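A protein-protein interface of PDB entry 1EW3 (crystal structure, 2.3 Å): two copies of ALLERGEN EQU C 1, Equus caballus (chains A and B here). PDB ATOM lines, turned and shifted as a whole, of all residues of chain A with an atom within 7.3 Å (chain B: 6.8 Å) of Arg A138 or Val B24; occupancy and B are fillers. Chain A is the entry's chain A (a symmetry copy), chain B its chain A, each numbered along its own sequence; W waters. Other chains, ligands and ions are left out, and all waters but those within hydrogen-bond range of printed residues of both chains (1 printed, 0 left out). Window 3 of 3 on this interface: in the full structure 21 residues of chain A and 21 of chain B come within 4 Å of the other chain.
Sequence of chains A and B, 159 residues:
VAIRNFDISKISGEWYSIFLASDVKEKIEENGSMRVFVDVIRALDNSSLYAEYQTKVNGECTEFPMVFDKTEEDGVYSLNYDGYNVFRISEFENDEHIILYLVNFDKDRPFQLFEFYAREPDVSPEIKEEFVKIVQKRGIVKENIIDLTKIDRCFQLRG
The side-chain amide nitrogen (NE2) of Gln A112 sits close to the side-chain amide nitrogen (NE2) of Gln B112 (3.5 Å). The backbone carbonyl oxygen (O) of Pro B110 lies within hydrogen-bond range of the guanidinium group (NH1) of Arg A138. The side-chain carboxylate of Asp B23 is in salt-bridge range of the guanidinium group of Arg A138, 2.9 Å away.
The side-chain hydroxyl of Ser B22 is in hydrogen-bond range of the backbone NH of Val B24 (3.0 Å). The side-chain hydroxyl (OG) of Ser B22 is in hydrogen-bond range of the backbone carbonyl oxygen (O) of Gln B112, 3.2 Å away. OD1 of Asp A23 is in hydrogen-bond range of NE2 of Gln A112, 2.5 Å away. The side-chain carboxylate (OD1) of Asp B23 sits at hydrogen-bond distance from the side-chain amide nitrogen (NE2) of Gln B112, 2.5 Å away. NH2 of Arg A138 lies within hydrogen-bond range of OE1 of Gln A112 (3.1 Å). The side-chain amide oxygen (OE1) of Gln A112 lies within hydrogen-bond range of the side-chain hydroxyl (OH) of Tyr A101 (3.0 Å).
Among the printed residues, merely in contact across the chains: Tyr A101 with Pro B110, Arg A138 with Val B24, Arg A138 with Phe B111 and Arg A138 with Gln B112.
Of the printed residues of chain B, Tyr A101 touches Pro B110. Printed residues of chain B within 4 Å of Gln A112: Gln B112 (3.5 Å). Printed residues of chain B within 4 Å of Arg A138: Asp B23, Val B24, Pro B110, Phe B111 and Gln B112. Of the printed residues of chain A, Asp B23 touches Arg A138 (2.9 Å). Of chain A, only Arg A138 comes within 4 Å of Val B24. Of the printed residues of chain A, Phe B111 touches Arg A138. Printed residues of chain A within 4 Å of Gln B112: Gln A112 (3.5 Å) and Arg A138 (3.99 Å). The nearest printed residue of chain B that does not touch Arg A138 is Arg B109 (5.6 Å). The nearest printed residue of chain A that does not touch Pro B110 is Lys A137 (6.0 Å).
Of the 15 printed residues of chain A, 3 touch a printed residue of chain B. Hydrophobic or aromatic side chains of chain A within 4 Å of the printed part of chain B: Tyr A101. Of the 16 printed residues of chain B, 5 touch a printed residue of chain A. Among the printed residues, Asp or Glu carboxylates within 4 Å of a Lys or Arg side-chain nitrogen of the other chain: Arg A138 with Asp B23.
Gln A112 touches its own counterpart, Gln B112.
Water W1 bridges the guanidinium group (NE) of Arg A138 (2.7 Å) and the backbone carbonyl oxygen (O) of Pro B110 (3.2 Å).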
ATOM      1  N   ASP A  23      -6.460  -4.757 -13.214  1.00  0.00           N
ATOM      2  CA  ASP A  23      -7.913  -4.500 -13.190  1.00  0.00           C
ATOM      3  C   ASP A  23      -8.476  -5.101 -14.451  1.00  0.00           C
ATOM      4  O   ASP A  23      -9.658  -5.012 -14.710  1.00  0.00           O
ATOM      5  CB  ASP A  23      -8.266  -3.040 -12.969  1.00  0.00           C
ATOM      6  CG  ASP A  23      -7.386  -2.073 -13.774  1.00  0.00           C
ATOM      7  OD1 ASP A  23      -7.197  -0.937 -13.269  1.00  0.00           O
ATOM      8  OD2 ASP A  23      -6.908  -2.489 -14.852  1.00  0.00           O
ATOM      9  N   TYR A 101       4.487  -0.954 -10.467  1.00  0.00           N
ATOM     10  CA  TYR A 101       3.205  -0.369 -10.862  1.00  0.00           C
ATOM     11  C   TYR A 101       3.373   0.139 -12.290  1.00  0.00           C
ATOM     12  O   TYR A 101       4.182   1.020 -12.578  1.00  0.00           O
ATOM     13  CB  TYR A 101       2.916   0.834  -9.929  1.00  0.00           C
ATOM     14  CG  TYR A 101       1.640   1.537 -10.380  1.00  0.00           C
ATOM     15  CD1 TYR A 101       0.408   0.889 -10.404  1.00  0.00           C
ATOM     16  CD2 TYR A 101       1.689   2.858 -10.781  1.00  0.00           C
ATOM     17  CE1 TYR A 101      -0.735   1.523 -10.870  1.00  0.00           C
ATOM     18  CE2 TYR A 101       0.546   3.505 -11.211  1.00  0.00           C
ATOM     19  CZ  TYR A 101      -0.658   2.856 -11.246  1.00  0.00           C
ATOM     20  OH  TYR A 101      -1.743   3.526 -11.736  1.00  0.00           O
ATOM     21  N   GLN A 112      -4.136  -1.175 -15.450  1.00  0.00           N
ATOM     22  CA  GLN A 112      -3.088  -1.057 -14.467  1.00  0.00           C
ATOM     23  C   GLN A 112      -2.670  -2.478 -14.022  1.00  0.00           C
ATOM     24  O   GLN A 112      -3.430  -3.461 -14.126  1.00  0.00           O
ATOM     25  CB  GLN A 112      -3.584  -0.238 -13.269  1.00  0.00           C
ATOM     26  CG  GLN A 112      -4.384   1.058 -13.516  1.00  0.00           C
ATOM     27  CD  GLN A 112      -4.996   1.431 -12.139  1.00  0.00           C
ATOM     28  OE1 GLN A 112      -4.372   2.087 -11.316  1.00  0.00           O
ATOM     29  NE2 GLN A 112      -6.166   0.843 -11.819  1.00  0.00           N
ATOM     30  N   LEU A 113      -1.403  -2.642 -13.675  1.00  0.00           N
ATOM     31  CA  LEU A 113      -0.871  -3.962 -13.377  1.00  0.00           C
ATOM     32  C   LEU A 113       0.156  -3.801 -12.290  1.00  0.00           C
ATOM     33  O   LEU A 113       0.879  -2.802 -12.363  1.00  0.00           O
ATOM     34  CB  LEU A 113      -0.312  -4.582 -14.670  1.00  0.00           C
ATOM     35  CG  LEU A 113       0.611  -5.824 -14.502  1.00  0.00           C
ATOM     36  CD1 LEU A 113      -0.200  -7.069 -14.828  1.00  0.00           C
ATOM     37  CD2 LEU A 113       1.776  -5.831 -15.480  1.00  0.00           C
ATOM     38  N   PHE A 114       0.178  -4.661 -11.287  1.00  0.00           N
ATOM     39  CA  PHE A 114       1.233  -4.691 -10.317  1.00  0.00           C
ATOM     40  C   PHE A 114       1.997  -6.025 -10.494  1.00  0.00           C
ATOM     41  O   PHE A 114       1.417  -7.011 -10.915  1.00  0.00           O
ATOM     42  CB  PHE A 114       0.822  -4.623  -8.852  1.00  0.00           C
ATOM     43  CG  PHE A 114       0.220  -3.317  -8.401  1.00  0.00           C
ATOM     44  CD1 PHE A 114      -1.078  -2.996  -8.700  1.00  0.00           C
ATOM     45  CD2 PHE A 114       0.963  -2.447  -7.639  1.00  0.00           C
ATOM     46  CE1 PHE A 114      -1.635  -1.807  -8.235  1.00  0.00           C
ATOM     47  CE2 PHE A 114       0.423  -1.258  -7.190  1.00  0.00           C
ATOM     48  CZ  PHE A 114      -0.870  -0.938  -7.495  1.00  0.00           C
ATOM     49  N   VAL A 132      -1.258  -7.174  -0.707  1.00  0.00           N
ATOM     50  CA  VAL A 132      -2.670  -7.151  -1.147  1.00  0.00           C
ATOM     51  C   VAL A 132      -3.359  -5.837  -0.774  1.00  0.00           C
ATOM     52  O   VAL A 132      -4.187  -5.318  -1.502  1.00  0.00           O
ATOM     53  CB  VAL A 132      -3.528  -8.330  -0.657  1.00  0.00           C
ATOM     54  CG1 VAL A 132      -3.137  -8.802   0.722  1.00  0.00           C
ATOM     55  CG2 VAL A 132      -5.010  -7.941  -0.584  1.00  0.00           C
ATOM     56  N   LYS A 133      -3.065  -5.351   0.410  1.00  0.00           N
ATOM     57  CA  LYS A 133      -3.585  -4.092   0.925  1.00  0.00           C
ATOM     58  C   LYS A 133      -3.245  -2.938  -0.028  1.00  0.00           C
ATOM     59  O   LYS A 133      -4.119  -2.400  -0.732  1.00  0.00           O
ATOM     60  CB  LYS A 133      -2.990  -3.951   2.318  1.00  0.00           C
ATOM     61  CG  LYS A 133      -2.210  -2.706   2.662  1.00  0.00           C
ATOM     62  CD  LYS A 133      -1.744  -2.806   4.125  1.00  0.00           C
ATOM     63  CE  LYS A 133      -2.039  -1.507   4.863  1.00  0.00           C
ATOM     64  NZ  LYS A 133      -1.101  -1.297   6.005  1.00  0.00           N
ATOM     65  N   ILE A 134      -1.952  -2.818  -0.346  1.00  0.00           N
ATOM     66  CA  ILE A 134      -1.518  -1.821  -1.309  1.00  0.00           C
ATOM     67  C   ILE A 134      -2.265  -1.905  -2.606  1.00  0.00           C
ATOM     68  O   ILE A 134      -2.735  -0.887  -3.093  1.00  0.00           O
ATOM     69  CB  ILE A 134      -0.017  -1.886  -1.623  1.00  0.00           C
ATOM     70  CG1 ILE A 134       0.744  -1.291  -0.445  1.00  0.00           C
ATOM     71  CG2 ILE A 134       0.239  -1.128  -2.928  1.00  0.00           C
ATOM     72  CD1 ILE A 134       2.093  -1.959  -0.302  1.00  0.00           C
ATOM     73  N   VAL A 135      -2.432  -3.141  -3.111  1.00  0.00           N
ATOM     74  CA  VAL A 135      -3.157  -3.249  -4.393  1.00  0.00           C
ATOM     75  C   VAL A 135      -4.600  -2.850  -4.227  1.00  0.00           C
ATOM     76  O   VAL A 135      -5.278  -2.404  -5.172  1.00  0.00           O
ATOM     77  CB  VAL A 135      -2.962  -4.667  -4.970  1.00  0.00           C
ATOM     78  CG1 VAL A 135      -3.979  -5.000  -6.045  1.00  0.00           C
ATOM     79  CG2 VAL A 135      -1.542  -4.863  -5.525  1.00  0.00           C
ATOM     80  N   GLN A 136      -5.143  -3.147  -3.032  1.00  0.00           N
ATOM     81  CA  GLN A 136      -6.577  -2.843  -2.807  1.00  0.00           C
ATOM     82  C   GLN A 136      -6.781  -1.329  -2.665  1.00  0.00           C
ATOM     83  O   GLN A 136      -7.699  -0.832  -3.321  1.00  0.00           O
ATOM     84  CB  GLN A 136      -7.126  -3.598  -1.604  1.00  0.00           C
ATOM     85  CG  GLN A 136      -7.335  -5.100  -1.829  1.00  0.00           C
ATOM     86  CD  GLN A 136      -7.999  -5.683  -0.576  1.00  0.00           C
ATOM     87  OE1 GLN A 136      -9.142  -6.143  -0.696  1.00  0.00           O
ATOM     88  NE2 GLN A 136      -7.316  -5.616   0.557  1.00  0.00           N
ATOM     89  N   LYS A 137      -5.849  -0.606  -2.061  1.00  0.00           N
ATOM     90  CA  LYS A 137      -5.895   0.848  -2.095  1.00  0.00           C
ATOM     91  C   LYS A 137      -5.927   1.418  -3.518  1.00  0.00           C
ATOM     92  O   LYS A 137      -6.511   2.493  -3.735  1.00  0.00           O
ATOM     93  CB  LYS A 137      -4.686   1.470  -1.385  1.00  0.00           C
ATOM     94  CG  LYS A 137      -3.942   2.430  -2.307  1.00  0.00           C
ATOM     95  CD  LYS A 137      -4.050   3.887  -1.892  1.00  0.00           C
ATOM     96  CE  LYS A 137      -2.715   4.381  -1.329  1.00  0.00           C
ATOM     97  NZ  LYS A 137      -2.020   3.274  -0.606  1.00  0.00           N
ATOM     98  N   ARG A 138      -5.263   0.757  -4.475  1.00  0.00           N
ATOM     99  CA  ARG A 138      -5.246   1.241  -5.850  1.00  0.00           C
ATOM    100  C   ARG A 138      -6.579   0.949  -6.494  1.00  0.00           C
ATOM    101  O   ARG A 138      -6.804   1.316  -7.659  1.00  0.00           O
ATOM    102  CB  ARG A 138      -4.113   0.635  -6.687  1.00  0.00           C
ATOM    103  CG  ARG A 138      -3.937   1.095  -8.123  1.00  0.00           C
ATOM    104  CD  ARG A 138      -3.128   2.389  -8.261  1.00  0.00           C
ATOM    105  NE  ARG A 138      -3.715   3.515  -7.538  1.00  0.00           N
ATOM    106  CZ  ARG A 138      -4.714   4.271  -7.989  1.00  0.00           C
ATOM    107  NH1 ARG A 138      -5.113   5.210  -7.145  1.00  0.00           N
ATOM    108  NH2 ARG A 138      -5.278   4.216  -9.179  1.00  0.00           N
ATOM    109  N   GLY A 139      -7.465   0.224  -5.785  1.00  0.00           N
ATOM    110  CA  GLY A 139      -8.789  -0.054  -6.337  1.00  0.00           C
ATOM    111  C   GLY A 139      -8.863  -1.322  -7.137  1.00  0.00           C
ATOM    112  O   GLY A 139      -9.698  -1.541  -8.025  1.00  0.00           O
ATOM    113  N   ILE A 140      -7.899  -2.215  -6.924  1.00  0.00           N
ATOM    114  CA  ILE A 140      -8.012  -3.469  -7.696  1.00  0.00           C
ATOM    115  C   ILE A 140      -8.641  -4.480  -6.748  1.00  0.00           C
ATOM    116  O   ILE A 140      -8.174  -4.529  -5.628  1.00  0.00           O
ATOM    117  CB  ILE A 140      -6.629  -3.881  -8.211  1.00  0.00           C
ATOM    118  CG1 ILE A 140      -6.291  -2.912  -9.382  1.00  0.00           C
ATOM    119  CG2 ILE A 140      -6.621  -5.302  -8.707  1.00  0.00           C
ATOM    120  CD1 ILE A 140      -4.814  -2.936  -9.678  1.00  0.00           C
ATOM    121  N   VAL A 141      -9.498  -5.379  -7.186  1.00  0.00           N
ATOM    122  CA  VAL A 141     -10.020  -6.316  -6.179  1.00  0.00           C
ATOM    123  C   VAL A 141      -9.180  -7.558  -5.991  1.00  0.00           C
ATOM    124  O   VAL A 141      -8.503  -7.995  -6.933  1.00  0.00           O
ATOM    125  CB  VAL A 141     -11.490  -6.608  -6.530  1.00  0.00           C
ATOM    126  CG1 VAL A 141     -11.646  -7.388  -7.806  1.00  0.00           C
ATOM    127  CG2 VAL A 141     -12.158  -7.201  -5.301  1.00  0.00           C
ATOM    128  N   ALA B  21     -12.662  13.365 -13.778  1.00  0.00           N
ATOM    129  CA  ALA B  21     -12.989  12.100 -13.078  1.00  0.00           C
ATOM    130  C   ALA B  21     -11.693  11.500 -12.585  1.00  0.00           C
ATOM    131  O   ALA B  21     -10.628  11.615 -13.228  1.00  0.00           O
ATOM    132  CB  ALA B  21     -13.799  11.164 -13.949  1.00  0.00           C
ATOM    133  N   SER B  22     -11.674  10.986 -11.365  1.00  0.00           N
ATOM    134  CA  SER B  22     -10.436  10.453 -10.817  1.00  0.00           C
ATOM    135  C   SER B  22     -10.649   9.478  -9.671  1.00  0.00           C
ATOM    136  O   SER B  22     -11.646   9.604  -8.967  1.00  0.00           O
ATOM    137  CB  SER B  22      -9.604  11.614 -10.386  1.00  0.00           C
ATOM    138  OG  SER B  22      -8.525  11.326  -9.525  1.00  0.00           O
ATOM    139  N   ASP B  23      -9.695   8.553  -9.474  1.00  0.00           N
ATOM    140  CA  ASP B  23      -9.951   7.573  -8.401  1.00  0.00           C
ATOM    141  C   ASP B  23      -9.399   8.169  -7.133  1.00  0.00           C
ATOM    142  O   ASP B  23      -9.446   7.560  -6.086  1.00  0.00           O
ATOM    143  CB  ASP B  23      -9.444   6.178  -8.722  1.00  0.00           C
ATOM    144  CG  ASP B  23      -8.053   6.172  -9.373  1.00  0.00           C
ATOM    145  OD1 ASP B  23      -7.807   5.221 -10.157  1.00  0.00           O
ATOM    146  OD2 ASP B  23      -7.282   7.117  -9.096  1.00  0.00           O
ATOM    147  N   VAL B  24      -8.867   9.393  -7.220  1.00  0.00           N
ATOM    148  CA  VAL B  24      -8.407  10.088  -6.016  1.00  0.00           C
ATOM    149  C   VAL B  24      -9.013  11.490  -6.075  1.00  0.00           C
ATOM    150  O   VAL B  24      -8.493  12.475  -6.628  1.00  0.00           O
ATOM    151  CB  VAL B  24      -6.896  10.098  -5.911  1.00  0.00           C
ATOM    152  CG1 VAL B  24      -6.431  10.897  -4.694  1.00  0.00           C
ATOM    153  CG2 VAL B  24      -6.295   8.700  -5.898  1.00  0.00           C
ATOM    154  N   LYS B  25     -10.282  11.536  -5.692  1.00  0.00           N
ATOM    155  CA  LYS B  25     -11.179  12.667  -5.670  1.00  0.00           C
ATOM    156  C   LYS B  25     -10.558  14.010  -5.295  1.00  0.00           C
ATOM    157  O   LYS B  25     -10.840  15.032  -5.898  1.00  0.00           O
ATOM    158  CB  LYS B  25     -12.324  12.451  -4.657  1.00  0.00           C
ATOM    159  CG  LYS B  25     -13.642  12.061  -5.309  1.00  0.00           C
ATOM    160  CD  LYS B  25     -14.225  13.162  -6.179  1.00  0.00           C
ATOM    161  CE  LYS B  25     -15.296  13.956  -5.434  1.00  0.00           C
ATOM    162  NZ  LYS B  25     -16.620  14.001  -6.152  1.00  0.00           N
ATOM    163  N   GLU B  26      -9.668  13.967  -4.347  1.00  0.00           N
ATOM    164  CA  GLU B  26      -9.091  15.158  -3.767  1.00  0.00           C
ATOM    165  C   GLU B  26      -8.290  15.915  -4.801  1.00  0.00           C
ATOM    166  O   GLU B  26      -8.032  17.111  -4.680  1.00  0.00           O
ATOM    167  CB  GLU B  26      -8.246  14.663  -2.603  1.00  0.00           C
ATOM    168  CG  GLU B  26      -7.599  15.609  -1.652  1.00  0.00           C
ATOM    169  CD  GLU B  26      -6.757  14.849  -0.629  1.00  0.00           C
ATOM    170  OE1 GLU B  26      -7.348  13.999   0.084  1.00  0.00           O
ATOM    171  OE2 GLU B  26      -5.527  15.071  -0.513  1.00  0.00           O
ATOM    172  N   LYS B  27      -7.788  15.217  -5.806  1.00  0.00           N
ATOM    173  CA  LYS B  27      -7.025  15.837  -6.880  1.00  0.00           C
ATOM    174  C   LYS B  27      -7.966  16.691  -7.708  1.00  0.00           C
ATOM    175  O   LYS B  27      -7.429  17.642  -8.281  1.00  0.00           O
ATOM    176  CB  LYS B  27      -6.379  14.714  -7.709  1.00  0.00           C
ATOM    177  CG  LYS B  27      -5.205  14.035  -6.968  1.00  0.00           C
ATOM    178  CD  LYS B  27      -4.157  15.130  -6.782  1.00  0.00           C
ATOM    179  CE  LYS B  27      -2.969  14.725  -5.968  1.00  0.00           C
ATOM    180  NZ  LYS B  27      -2.036  15.876  -5.745  1.00  0.00           N
ATOM    181  N   ILE B  28      -9.248  16.316  -7.879  1.00  0.00           N
ATOM    182  CA  ILE B  28     -10.090  17.191  -8.685  1.00  0.00           C
ATOM    183  C   ILE B  28     -11.108  18.070  -7.940  1.00  0.00           C
ATOM    184  O   ILE B  28     -11.988  18.661  -8.587  1.00  0.00           O
ATOM    185  CB  ILE B  28     -10.849  16.397  -9.752  1.00  0.00           C
ATOM    186  CG1 ILE B  28     -11.494  15.191  -9.065  1.00  0.00           C
ATOM    187  CG2 ILE B  28      -9.825  16.013 -10.818  1.00  0.00           C
ATOM    188  CD1 ILE B  28     -12.466  14.442  -9.954  1.00  0.00           C
ATOM    189  N   GLU B  29     -10.964  18.154  -6.615  1.00  0.00           N
ATOM    190  CA  GLU B  29     -11.843  18.934  -5.785  1.00  0.00           C
ATOM    191  C   GLU B  29     -11.216  20.311  -5.539  1.00  0.00           C
ATOM    192  O   GLU B  29     -10.030  20.574  -5.819  1.00  0.00           O
ATOM    193  CB  GLU B  29     -12.131  18.229  -4.451  1.00  0.00           C
ATOM    194  CG  GLU B  29     -13.290  17.246  -4.480  1.00  0.00           C
ATOM    195  CD  GLU B  29     -13.412  16.433  -3.201  1.00  0.00           C
ATOM    196  OE1 GLU B  29     -14.493  15.821  -2.996  1.00  0.00           O
ATOM    197  OE2 GLU B  29     -12.476  16.377  -2.370  1.00  0.00           O
ATOM    198  N   ARG B 109       1.111   7.821  -3.967  1.00  0.00           N
ATOM    199  CA  ARG B 109      -0.298   7.855  -4.313  1.00  0.00           C
ATOM    200  C   ARG B 109      -0.539   8.192  -5.782  1.00  0.00           C
ATOM    201  O   ARG B 109      -0.915   9.322  -6.085  1.00  0.00           O
ATOM    202  CB  ARG B 109      -0.946   8.916  -3.416  1.00  0.00           C
ATOM    203  N   PRO B 110      -0.373   7.210  -6.660  1.00  0.00           N
ATOM    204  CA  PRO B 110      -0.574   7.415  -8.080  1.00  0.00           C
ATOM    205  C   PRO B 110      -2.066   7.531  -8.304  1.00  0.00           C
ATOM    206  O   PRO B 110      -2.799   7.082  -7.411  1.00  0.00           O
ATOM    207  CB  PRO B 110      -0.020   6.158  -8.746  1.00  0.00           C
ATOM    208  CG  PRO B 110      -0.145   5.126  -7.669  1.00  0.00           C
ATOM    209  CD  PRO B 110       0.121   5.832  -6.369  1.00  0.00           C
ATOM    210  N   PHE B 111      -2.480   8.067  -9.465  1.00  0.00           N
ATOM    211  CA  PHE B 111      -3.935   8.003  -9.645  1.00  0.00           C
ATOM    212  C   PHE B 111      -4.190   8.114 -11.132  1.00  0.00           C
ATOM    213  O   PHE B 111      -3.278   8.515 -11.858  1.00  0.00           O
ATOM    214  CB  PHE B 111      -4.544   9.239  -8.951  1.00  0.00           C
ATOM    215  CG  PHE B 111      -4.045  10.599  -9.343  1.00  0.00           C
ATOM    216  CD1 PHE B 111      -4.576  11.296 -10.409  1.00  0.00           C
ATOM    217  CD2 PHE B 111      -3.050  11.210  -8.622  1.00  0.00           C
ATOM    218  CE1 PHE B 111      -4.162  12.587 -10.713  1.00  0.00           C
ATOM    219  CE2 PHE B 111      -2.615  12.484  -8.907  1.00  0.00           C
ATOM    220  CZ  PHE B 111      -3.189  13.176  -9.961  1.00  0.00           C
ATOM    221  N   GLN B 112      -5.387   7.778 -11.492  1.00  0.00           N
ATOM    222  CA  GLN B 112      -5.847   7.909 -12.853  1.00  0.00           C
ATOM    223  C   GLN B 112      -6.855   9.081 -12.920  1.00  0.00           C
ATOM    224  O   GLN B 112      -7.491   9.473 -11.921  1.00  0.00           O
ATOM    225  CB  GLN B 112      -6.506   6.602 -13.310  1.00  0.00           C
ATOM    226  CG  GLN B 112      -5.823   5.256 -12.988  1.00  0.00           C
ATOM    227  CD  GLN B 112      -6.893   4.171 -13.287  1.00  0.00           C
ATOM    228  OE1 GLN B 112      -7.046   3.714 -14.411  1.00  0.00           O
ATOM    229  NE2 GLN B 112      -7.764   3.896 -12.296  1.00  0.00           N
ATOM    230  N   LEU B 113      -6.897   9.763 -14.053  1.00  0.00           N
ATOM    231  CA  LEU B 113      -7.703  10.967 -14.175  1.00  0.00           C
ATOM    232  C   LEU B 113      -8.230  11.018 -15.582  1.00  0.00           C
ATOM    233  O   LEU B 113      -7.454  10.654 -16.472  1.00  0.00           O
ATOM    234  CB  LEU B 113      -6.847  12.187 -13.790  1.00  0.00           C
ATOM    235  CG  LEU B 113      -7.405  13.583 -14.191  1.00  0.00           C
ATOM    236  CD1 LEU B 113      -8.014  14.227 -12.954  1.00  0.00           C
ATOM    237  CD2 LEU B 113      -6.321  14.542 -14.657  1.00  0.00           C
ATOM    238  N   ILE B 140     -13.786   3.670 -12.216  1.00  0.00           N
ATOM    239  CA  ILE B 140     -13.860   4.846 -11.324  1.00  0.00           C
ATOM    240  C   ILE B 140     -15.324   4.970 -10.929  1.00  0.00           C
ATOM    241  O   ILE B 140     -16.134   4.874 -11.830  1.00  0.00           O
ATOM    242  CB  ILE B 140     -13.308   6.077 -12.050  1.00  0.00           C
ATOM    243  CG1 ILE B 140     -11.761   5.905 -12.089  1.00  0.00           C
ATOM    244  CG2 ILE B 140     -13.662   7.351 -11.332  1.00  0.00           C
ATOM    245  CD1 ILE B 140     -11.154   6.811 -13.129  1.00  0.00           C
ATOM    246  N   ASN B 144     -17.139  10.121  -8.130  1.00  0.00           N
ATOM    247  CA  ASN B 144     -15.896  10.780  -8.456  1.00  0.00           C
ATOM    248  C   ASN B 144     -15.879  11.562  -9.761  1.00  0.00           C
ATOM    249  O   ASN B 144     -14.817  11.965 -10.231  1.00  0.00           O
ATOM    250  CB  ASN B 144     -14.750   9.749  -8.436  1.00  0.00           C
ATOM    251  CG  ASN B 144     -14.526   9.292  -7.010  1.00  0.00           C
ATOM    252  OD1 ASN B 144     -13.399   9.044  -6.576  1.00  0.00           O
ATOM    253  ND2 ASN B 144     -15.668   9.197  -6.330  1.00  0.00           N
HETATM  254  O   HOH W   1      -3.000   4.745  -5.250  1.00  0.00           O
